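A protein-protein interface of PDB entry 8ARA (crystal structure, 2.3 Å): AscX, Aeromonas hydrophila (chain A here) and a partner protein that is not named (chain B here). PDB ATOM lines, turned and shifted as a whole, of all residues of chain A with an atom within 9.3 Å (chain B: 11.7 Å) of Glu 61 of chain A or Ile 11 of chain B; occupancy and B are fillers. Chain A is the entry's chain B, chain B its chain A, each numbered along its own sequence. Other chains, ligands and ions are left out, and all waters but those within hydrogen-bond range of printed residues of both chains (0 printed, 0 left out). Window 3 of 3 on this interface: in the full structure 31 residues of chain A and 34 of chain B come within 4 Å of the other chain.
O of Leu 13 of chain B lies within hydrogen-bond range of NE2 of Gln 18 of chain B (3.1 Å). The side-chain amide oxygen of Gln 17 of chain B lies within hydrogen-bond range of the backbone NH of Thr 14 of chain B, at 3.1 Å. O of Asp 42 of chain B sits at hydrogen-bond distance from OG1 of Thr 46 of chain B. OG of Ser 64 of chain A sits close to N of Leu 67 of chain A, at 3.4 Å.
O of Gly 54 of chain A touches NE2 of Gln 17 of chain B (3.9 Å). Leu 55 of chain A touches Leu 13 of chain B (CD1 to CD2, 3.7 Å). Leu 55 of chain A touches Leu 21 of chain B (CD2 to CD1, 3.9 Å). CG1 of Val 58 of chain A touches CG2 of Ile 11 of chain B, at 3.7 Å. Thr 12 of chain B touches Val 58 of chain A. CG1 of Val 58 of chain A touches CD2 of Leu 13 of chain B, 3.7 Å away. Val 58 of chain A touches Gln 17 of chain B. Glu 61 of chain A touches Ile 11 of chain B (CB to CD1, 3.7 Å). Leu 67 of chain A touches Thr 46 of chain B (CD1 to CG2, 3.8 Å). CD2 of Leu 67 of chain A touches CD2 of Leu 47 of chain B (3.9 Å).
Glu 61 of chain A touches one residue of chain B. Printed residues of chain A within 4 Å of Ile 11 of chain B: Val 58 (3.7 Å) and Glu 61 (3.7 Å). Val 58 of chain A touches just these residues of chain B: Ile 11, Thr 12, Leu 13 and Gln 17. No residue of chain B comes within 4 Å of Ala 60 of chain A. No residue of chain B comes within 4 Å of Gly 62 of chain A. No residue of chain B comes within 4 Å of Gln 63 of chain A. Asn 10 of chain B touches none of the printed residues of chain A. Thr 12 of chain B touches just one residue of chain A: Val 58 (3.6 Å). Of the printed residues of chain A, Thr 46 of chain B touches Leu 67 (3.8 Å). Printed residues of chain B within 4 Å of Leu 55 of chain A: Leu 13 (3.7 Å) and Leu 21 (3.9 Å). Printed residues of chain B within 4 Å of Leu 67 of chain A: Thr 46 (3.8 Å) and Leu 47 (3.9 Å). Printed residues of chain A within 4 Å of Leu 13 of chain B: Leu 55 and Val 58. Of the printed residues of chain A, Leu 21 of chain B touches Leu 55 (3.9 Å). The nearest residue of chain B that does not touch Glu 61 of chain A is Asn 10 of chain B (5.9 Å). The nearest residue of chain A that does not touch Ile 11 of chain B is Leu 67 of chain A (4.1 Å). The nearest printed residue of chain A that does not touch Leu 21 of chain B is Leu 59 of chain A (4.7 Å).
Hydrophobic or aromatic side chains of chain A that line the printed part of chain B: Leu 55, Val 58 and Leu 67. Hydrophobic or aromatic side chains of chain B that line the printed part of chain A: Ile 11, Leu 13, Leu 21 and Leu 47. Among the printed residues, 10 pairs touch across the chains.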
ATOM      1  N   GLY A  54      -2.068  18.369   6.337  1.00  0.00           N
ATOM      2  CA  GLY A  54      -1.573  17.045   6.655  1.00  0.00           C
ATOM      3  C   GLY A  54      -0.747  16.465   5.530  1.00  0.00           C
ATOM      4  O   GLY A  54       0.288  15.837   5.765  1.00  0.00           O
ATOM      5  N   LEU A  55      -1.207  16.675   4.294  1.00  0.00           N
ATOM      6  CA  LEU A  55      -0.485  16.182   3.125  1.00  0.00           C
ATOM      7  C   LEU A  55       0.841  16.909   2.947  1.00  0.00           C
ATOM      8  O   LEU A  55       1.876  16.277   2.702  1.00  0.00           O
ATOM      9  CB  LEU A  55      -1.356  16.339   1.881  1.00  0.00           C
ATOM     10  CG  LEU A  55      -0.756  15.928   0.541  1.00  0.00           C
ATOM     11  CD1 LEU A  55      -0.478  14.438   0.529  1.00  0.00           C
ATOM     12  CD2 LEU A  55      -1.697  16.316  -0.582  1.00  0.00           C
ATOM     13  N   ARG A  56       0.829  18.239   3.058  1.00  0.00           N
ATOM     14  CA  ARG A  56       2.078  18.987   3.061  1.00  0.00           C
ATOM     15  C   ARG A  56       3.019  18.486   4.149  1.00  0.00           C
ATOM     16  O   ARG A  56       4.234  18.428   3.937  1.00  0.00           O
ATOM     17  CB  ARG A  56       1.796  20.477   3.244  1.00  0.00           C
ATOM     18  CG  ARG A  56       1.003  21.098   2.103  1.00  0.00           C
ATOM     19  CD  ARG A  56       0.647  22.542   2.404  1.00  0.00           C
ATOM     20  NE  ARG A  56       1.840  23.355   2.593  1.00  0.00           N
ATOM     21  CZ  ARG A  56       1.828  24.624   2.978  1.00  0.00           C
ATOM     22  NH1 ARG A  56       0.697  25.251   3.251  1.00  0.00           N
ATOM     23  NH2 ARG A  56       2.981  25.278   3.089  1.00  0.00           N
ATOM     24  N   SER A  57       2.475  18.104   5.308  1.00  0.00           N
ATOM     25  CA  SER A  57       3.315  17.596   6.388  1.00  0.00           C
ATOM     26  C   SER A  57       4.060  16.339   5.965  1.00  0.00           C
ATOM     27  O   SER A  57       5.245  16.176   6.274  1.00  0.00           O
ATOM     28  CB  SER A  57       2.467  17.316   7.627  1.00  0.00           C
ATOM     29  OG  SER A  57       3.208  16.591   8.590  1.00  0.00           O
ATOM     30  N   VAL A  58       3.385  15.444   5.250  1.00  0.00           N
ATOM     31  CA  VAL A  58       3.995  14.177   4.866  1.00  0.00           C
ATOM     32  C   VAL A  58       4.949  14.366   3.694  1.00  0.00           C
ATOM     33  O   VAL A  58       6.072  13.848   3.699  1.00  0.00           O
ATOM     34  CB  VAL A  58       2.901  13.144   4.548  1.00  0.00           C
ATOM     35  CG1 VAL A  58       3.516  11.872   4.008  1.00  0.00           C
ATOM     36  CG2 VAL A  58       2.084  12.855   5.798  1.00  0.00           C
ATOM     37  N   LEU A  59       4.526  15.114   2.672  1.00  0.00           N
ATOM     38  CA  LEU A  59       5.383  15.313   1.509  1.00  0.00           C
ATOM     39  C   LEU A  59       6.628  16.122   1.844  1.00  0.00           C
ATOM     40  O   LEU A  59       7.620  16.043   1.114  1.00  0.00           O
ATOM     41  CB  LEU A  59       4.606  15.998   0.386  1.00  0.00           C
ATOM     42  CG  LEU A  59       3.366  15.288  -0.158  1.00  0.00           C
ATOM     43  CD1 LEU A  59       2.771  16.099  -1.291  1.00  0.00           C
ATOM     44  CD2 LEU A  59       3.698  13.887  -0.622  1.00  0.00           C
ATOM     45  N   ALA A  60       6.599  16.890   2.937  1.00  0.00           N
ATOM     46  CA  ALA A  60       7.754  17.682   3.342  1.00  0.00           C
ATOM     47  C   ALA A  60       8.932  16.825   3.780  1.00  0.00           C
ATOM     48  O   ALA A  60      10.059  17.326   3.836  1.00  0.00           O
ATOM     49  CB  ALA A  60       7.367  18.630   4.477  1.00  0.00           C
ATOM     50  N   GLU A  61       8.706  15.554   4.096  1.00  0.00           N
ATOM     51  CA  GLU A  61       9.787  14.685   4.528  1.00  0.00           C
ATOM     52  C   GLU A  61      10.408  13.887   3.390  1.00  0.00           C
ATOM     53  O   GLU A  61      11.488  13.316   3.575  1.00  0.00           O
ATOM     54  CB  GLU A  61       9.288  13.725   5.604  1.00  0.00           C
ATOM     55  CG  GLU A  61       8.504  14.407   6.692  1.00  0.00           C
ATOM     56  CD  GLU A  61       8.224  13.484   7.847  1.00  0.00           C
ATOM     57  OE1 GLU A  61       8.986  12.505   8.009  1.00  0.00           O
ATOM     58  OE2 GLU A  61       7.245  13.734   8.584  1.00  0.00           O
ATOM     59  N   GLY A  62       9.760  13.835   2.230  1.00  0.00           N
ATOM     60  CA  GLY A  62      10.308  13.083   1.116  1.00  0.00           C
ATOM     61  C   GLY A  62      11.539  13.760   0.543  1.00  0.00           C
ATOM     62  O   GLY A  62      11.596  14.981   0.392  1.00  0.00           O
ATOM     63  N   GLN A  63      12.543  12.948   0.225  1.00  0.00           N
ATOM     64  CA  GLN A  63      13.794  13.453  -0.321  1.00  0.00           C
ATOM     65  C   GLN A  63      13.903  13.280  -1.828  1.00  0.00           C
ATOM     66  O   GLN A  63      14.779  13.896  -2.443  1.00  0.00           O
ATOM     67  CB  GLN A  63      14.981  12.767   0.366  1.00  0.00           C
ATOM     68  CG  GLN A  63      15.044  13.022   1.865  1.00  0.00           C
ATOM     69  CD  GLN A  63      16.218  12.335   2.535  1.00  0.00           C
ATOM     70  OE1 GLN A  63      16.966  11.591   1.898  1.00  0.00           O
ATOM     71  NE2 GLN A  63      16.386  12.582   3.828  1.00  0.00           N
ATOM     72  N   SER A  64      13.038  12.465  -2.437  1.00  0.00           N
ATOM     73  CA  SER A  64      13.058  12.294  -3.879  1.00  0.00           C
ATOM     74  C   SER A  64      12.701  13.611  -4.562  1.00  0.00           C
ATOM     75  O   SER A  64      12.079  14.487  -3.955  1.00  0.00           O
ATOM     76  CB  SER A  64      12.077  11.199  -4.295  1.00  0.00           C
ATOM     77  OG  SER A  64      10.739  11.597  -4.059  1.00  0.00           O
ATOM     78  N   LEU A  67       8.675  14.216  -4.647  1.00  0.00           N
ATOM     79  CA  LEU A  67       8.040  14.715  -3.433  1.00  0.00           C
ATOM     80  C   LEU A  67       8.511  16.127  -3.105  1.00  0.00           C
ATOM     81  O   LEU A  67       7.720  16.963  -2.656  1.00  0.00           O
ATOM     82  CB  LEU A  67       8.309  13.760  -2.267  1.00  0.00           C
ATOM     83  CG  LEU A  67       7.366  12.556  -2.143  1.00  0.00           C
ATOM     84  CD1 LEU A  67       7.538  11.552  -3.277  1.00  0.00           C
ATOM     85  CD2 LEU A  67       7.538  11.872  -0.797  1.00  0.00           C
ATOM     86  N   ARG A  68       9.793  16.419  -3.335  1.00  0.00           N
ATOM     87  CA  ARG A  68      10.295  17.764  -3.078  1.00  0.00           C
ATOM     88  C   ARG A  68       9.692  18.780  -4.042  1.00  0.00           C
ATOM     89  O   ARG A  68       9.505  19.948  -3.675  1.00  0.00           O
ATOM     90  CB  ARG A  68      11.823  17.775  -3.159  1.00  0.00           C
ATOM     91  CG  ARG A  68      12.460  19.128  -2.862  1.00  0.00           C
ATOM     92  CD  ARG A  68      13.979  19.087  -2.994  1.00  0.00           C
ATOM     93  NE  ARG A  68      14.616  18.393  -1.881  1.00  0.00           N
ATOM     94  CZ  ARG A  68      14.986  17.118  -1.899  1.00  0.00           C
ATOM     95  NH1 ARG A  68      14.796  16.359  -2.968  1.00  0.00           N
ATOM     96  NH2 ARG A  68      15.559  16.594  -0.819  1.00  0.00           N
ATOM     97  N   ALA A  71       5.957  19.254  -2.797  1.00  0.00           N
ATOM     98  CA  ALA A  71       5.889  20.002  -1.549  1.00  0.00           C
ATOM     99  C   ALA A  71       6.070  21.496  -1.795  1.00  0.00           C
ATOM    100  O   ALA A  71       5.379  22.319  -1.185  1.00  0.00           O
ATOM    101  CB  ALA A  71       6.935  19.481  -0.564  1.00  0.00           C
ATOM    102  N   ASN B  10      11.503   6.286   5.038  1.00  0.00           N
ATOM    103  CA  ASN B  10      10.296   5.649   4.525  1.00  0.00           C
ATOM    104  C   ASN B  10       9.087   6.576   4.673  1.00  0.00           C
ATOM    105  O   ASN B  10       8.797   7.058   5.769  1.00  0.00           O
ATOM    106  CB  ASN B  10      10.045   4.325   5.249  1.00  0.00           C
ATOM    107  CG  ASN B  10       9.038   3.449   4.530  1.00  0.00           C
ATOM    108  OD1 ASN B  10       8.879   3.537   3.311  1.00  0.00           O
ATOM    109  ND2 ASN B  10       8.354   2.596   5.283  1.00  0.00           N
ATOM    110  N   ILE B  11       8.386   6.818   3.566  1.00  0.00           N
ATOM    111  CA  ILE B  11       7.245   7.726   3.523  1.00  0.00           C
ATOM    112  C   ILE B  11       6.034   6.967   2.998  1.00  0.00           C
ATOM    113  O   ILE B  11       6.150   6.163   2.067  1.00  0.00           O
ATOM    114  CB  ILE B  11       7.529   8.959   2.640  1.00  0.00           C
ATOM    115  CG1 ILE B  11       8.791   9.685   3.111  1.00  0.00           C
ATOM    116  CG2 ILE B  11       6.332   9.900   2.623  1.00  0.00           C
ATOM    117  CD1 ILE B  11       8.716  10.180   4.534  1.00  0.00           C
ATOM    118  N   THR B  12       4.871   7.226   3.593  1.00  0.00           N
ATOM    119  CA  THR B  12       3.628   6.595   3.178  1.00  0.00           C
ATOM    120  C   THR B  12       2.484   7.592   3.291  1.00  0.00           C
ATOM    121  O   THR B  12       2.486   8.467   4.161  1.00  0.00           O
ATOM    122  CB  THR B  12       3.296   5.362   4.025  1.00  0.00           C
ATOM    123  OG1 THR B  12       3.434   5.692   5.409  1.00  0.00           O
ATOM    124  CG2 THR B  12       4.214   4.201   3.684  1.00  0.00           C
ATOM    125  N   LEU B  13       1.504   7.444   2.403  1.00  0.00           N
ATOM    126  CA  LEU B  13       0.257   8.189   2.465  1.00  0.00           C
ATOM    127  C   LEU B  13      -0.876   7.252   2.852  1.00  0.00           C
ATOM    128  O   LEU B  13      -0.927   6.103   2.400  1.00  0.00           O
ATOM    129  CB  LEU B  13      -0.069   8.854   1.127  1.00  0.00           C
ATOM    130  CG  LEU B  13       0.866   9.946   0.610  1.00  0.00           C
ATOM    131  CD1 LEU B  13       0.417  10.398  -0.769  1.00  0.00           C
ATOM    132  CD2 LEU B  13       0.907  11.113   1.570  1.00  0.00           C
ATOM    133  N   THR B  14      -1.781   7.743   3.692  1.00  0.00           N
ATOM    134  CA  THR B  14      -2.969   6.977   4.022  1.00  0.00           C
ATOM    135  C   THR B  14      -3.925   6.960   2.830  1.00  0.00           C
ATOM    136  O   THR B  14      -3.722   7.644   1.826  1.00  0.00           O
ATOM    137  CB  THR B  14      -3.660   7.561   5.253  1.00  0.00           C
ATOM    138  OG1 THR B  14      -4.057   8.911   4.984  1.00  0.00           O
ATOM    139  CG2 THR B  14      -2.726   7.539   6.452  1.00  0.00           C
ATOM    140  N   LYS B  15      -4.985   6.159   2.951  1.00  0.00           N
ATOM    141  CA  LYS B  15      -5.938   6.029   1.855  1.00  0.00           C
ATOM    142  C   LYS B  15      -6.606   7.365   1.548  1.00  0.00           C
ATOM    143  O   LYS B  15      -6.689   7.778   0.385  1.00  0.00           O
ATOM    144  CB  LYS B  15      -6.978   4.961   2.190  1.00  0.00           C
ATOM    145  CG  LYS B  15      -6.378   3.594   2.480  1.00  0.00           C
ATOM    146  CD  LYS B  15      -7.412   2.630   3.041  1.00  0.00           C
ATOM    147  CE  LYS B  15      -6.762   1.330   3.498  1.00  0.00           C
ATOM    148  NZ  LYS B  15      -7.755   0.361   4.041  1.00  0.00           N
ATOM    149  N   GLN B  17      -5.470  10.318   2.236  1.00  0.00           N
ATOM    150  CA  GLN B  17      -4.466  11.243   1.720  1.00  0.00           C
ATOM    151  C   GLN B  17      -4.164  10.969   0.251  1.00  0.00           C
ATOM    152  O   GLN B  17      -3.967  11.906  -0.531  1.00  0.00           O
ATOM    153  CB  GLN B  17      -3.190  11.161   2.562  1.00  0.00           C
ATOM    154  CG  GLN B  17      -3.294  11.857   3.914  1.00  0.00           C
ATOM    155  CD  GLN B  17      -2.061  11.663   4.780  1.00  0.00           C
ATOM    156  OE1 GLN B  17      -1.333  10.679   4.637  1.00  0.00           O
ATOM    157  NE2 GLN B  17      -1.824  12.603   5.689  1.00  0.00           N
ATOM    158  N   GLN B  18      -4.124   9.693  -0.144  1.00  0.00           N
ATOM    159  CA  GLN B  18      -3.938   9.370  -1.556  1.00  0.00           C
ATOM    160  C   GLN B  18      -5.075   9.929  -2.401  1.00  0.00           C
ATOM    161  O   GLN B  18      -4.852  10.391  -3.525  1.00  0.00           O
ATOM    162  CB  GLN B  18      -3.834   7.859  -1.749  1.00  0.00           C
ATOM    163  CG  GLN B  18      -2.594   7.232  -1.151  1.00  0.00           C
ATOM    164  CD  GLN B  18      -2.584   5.725  -1.311  1.00  0.00           C
ATOM    165  OE1 GLN B  18      -2.965   5.196  -2.355  1.00  0.00           O
ATOM    166  NE2 GLN B  18      -2.159   5.024  -0.267  1.00  0.00           N
ATOM    167  N   LEU B  21      -4.707  13.832  -2.503  1.00  0.00           N
ATOM    168  CA  LEU B  21      -3.678  14.203  -3.466  1.00  0.00           C
ATOM    169  C   LEU B  21      -4.134  13.943  -4.898  1.00  0.00           C
ATOM    170  O   LEU B  21      -3.770  14.693  -5.808  1.00  0.00           O
ATOM    171  CB  LEU B  21      -2.382  13.450  -3.159  1.00  0.00           C
ATOM    172  CG  LEU B  21      -1.168  13.695  -4.060  1.00  0.00           C
ATOM    173  CD1 LEU B  21      -0.830  15.179  -4.165  1.00  0.00           C
ATOM    174  CD2 LEU B  21       0.020  12.914  -3.528  1.00  0.00           C
ATOM    175  N   ASP B  42       2.835  12.840  -9.978  1.00  0.00           N
ATOM    176  CA  ASP B  42       4.124  12.157  -9.894  1.00  0.00           C
ATOM    177  C   ASP B  42       4.455  11.790  -8.453  1.00  0.00           C
ATOM    178  O   ASP B  42       4.976  10.701  -8.187  1.00  0.00           O
ATOM    179  CB  ASP B  42       5.238  13.034 -10.470  1.00  0.00           C
ATOM    180  CG  ASP B  42       5.400  12.883 -11.972  1.00  0.00           C
ATOM    181  OD1 ASP B  42       5.094  11.799 -12.514  1.00  0.00           O
ATOM    182  OD2 ASP B  42       5.857  13.858 -12.609  1.00  0.00           O
ATOM    183  N   ALA B  43       4.176  12.693  -7.510  1.00  0.00           N
ATOM    184  CA  ALA B  43       4.419  12.385  -6.105  1.00  0.00           C
ATOM    185  C   ALA B  43       3.481  11.289  -5.619  1.00  0.00           C
ATOM    186  O   ALA B  43       3.896  10.393  -4.875  1.00  0.00           O
ATOM    187  CB  ALA B  43       4.270  13.645  -5.254  1.00  0.00           C
ATOM    188  N   LEU B  44       2.213  11.343  -6.030  1.00  0.00           N
ATOM    189  CA  LEU B  44       1.276  10.277  -5.692  1.00  0.00           C
ATOM    190  C   LEU B  44       1.784   8.929  -6.184  1.00  0.00           C
ATOM    191  O   LEU B  44       1.872   7.965  -5.415  1.00  0.00           O
ATOM    192  CB  LEU B  44      -0.100  10.580  -6.289  1.00  0.00           C
ATOM    193  CG  LEU B  44      -1.138   9.461  -6.225  1.00  0.00           C
ATOM    194  CD1 LEU B  44      -1.478   9.134  -4.780  1.00  0.00           C
ATOM    195  CD2 LEU B  44      -2.387   9.848  -7.003  1.00  0.00           C
ATOM    196  N   LEU B  45       2.144   8.849  -7.462  1.00  0.00           N
ATOM    197  CA  LEU B  45       2.558   7.592  -8.067  1.00  0.00           C
ATOM    198  C   LEU B  45       3.973   7.179  -7.685  1.00  0.00           C
ATOM    199  O   LEU B  45       4.347   6.026  -7.923  1.00  0.00           O
ATOM    200  CB  LEU B  45       2.420   7.691  -9.586  1.00  0.00           C
ATOM    201  CG  LEU B  45       0.967   7.841 -10.041  1.00  0.00           C
ATOM    202  CD1 LEU B  45       0.878   8.155 -11.523  1.00  0.00           C
ATOM    203  CD2 LEU B  45       0.191   6.577  -9.714  1.00  0.00           C
ATOM    204  N   THR B  46       4.769   8.079  -7.105  1.00  0.00           N
ATOM    205  CA  THR B  46       6.036   7.652  -6.517  1.00  0.00           C
ATOM    206  C   THR B  46       5.795   6.850  -5.244  1.00  0.00           C
ATOM    207  O   THR B  46       6.460   5.836  -5.005  1.00  0.00           O
ATOM    208  CB  THR B  46       6.927   8.865  -6.231  1.00  0.00           C
ATOM    209  OG1 THR B  46       7.379   9.432  -7.466  1.00  0.00           O
ATOM    210  CG2 THR B  46       8.137   8.469  -5.404  1.00  0.00           C
ATOM    211  N   LEU B  47       4.830   7.277  -4.428  1.00  0.00           N
ATOM    212  CA  LEU B  47       4.523   6.606  -3.173  1.00  0.00           C
ATOM    213  C   LEU B  47       3.556   5.441  -3.337  1.00  0.00           C
ATOM    214  O   LEU B  47       3.537   4.543  -2.487  1.00  0.00           O
ATOM    215  CB  LEU B  47       3.947   7.614  -2.176  1.00  0.00           C
ATOM    216  CG  LEU B  47       4.876   8.787  -1.860  1.00  0.00           C
ATOM    217  CD1 LEU B  47       4.184   9.807  -0.970  1.00  0.00           C
ATOM    218  CD2 LEU B  47       6.162   8.282  -1.214  1.00  0.00           C
ATOM    219  N   ASN B  48       2.754   5.434  -4.395  1.00  0.00           N
ATOM    220  CA  ASN B  48       1.866   4.313  -4.707  1.00  0.00           C
ATOM    221  C   ASN B  48       1.796   4.181  -6.220  1.00  0.00           C
ATOM    222  O   ASN B  48       0.871   4.687  -6.867  1.00  0.00           O
ATOM    223  CB  ASN B  48       0.479   4.514  -4.093  1.00  0.00           C
ATOM    224  CG  ASN B  48      -0.396   3.277  -4.210  1.00  0.00           C
ATOM    225  OD1 ASN B  48       0.094   2.167  -4.437  1.00  0.00           O
ATOM    226  ND2 ASN B  48      -1.703   3.462  -4.051  1.00  0.00           N
ATOM    227  N   PRO B  49       2.777   3.505  -6.828  1.00  0.00           N
ATOM    228  CA  PRO B  49       2.792   3.385  -8.294  1.00  0.00           C
ATOM    229  C   PRO B  49       1.690   2.505  -8.861  1.00  0.00           C
ATOM    230  O   PRO B  49       1.509   2.494 -10.084  1.00  0.00           O
ATOM    231  CB  PRO B  49       4.179   2.792  -8.582  1.00  0.00           C
ATOM    232  CG  PRO B  49       4.554   2.085  -7.322  1.00  0.00           C
ATOM    233  CD  PRO B  49       3.959   2.888  -6.204  1.00  0.00           C
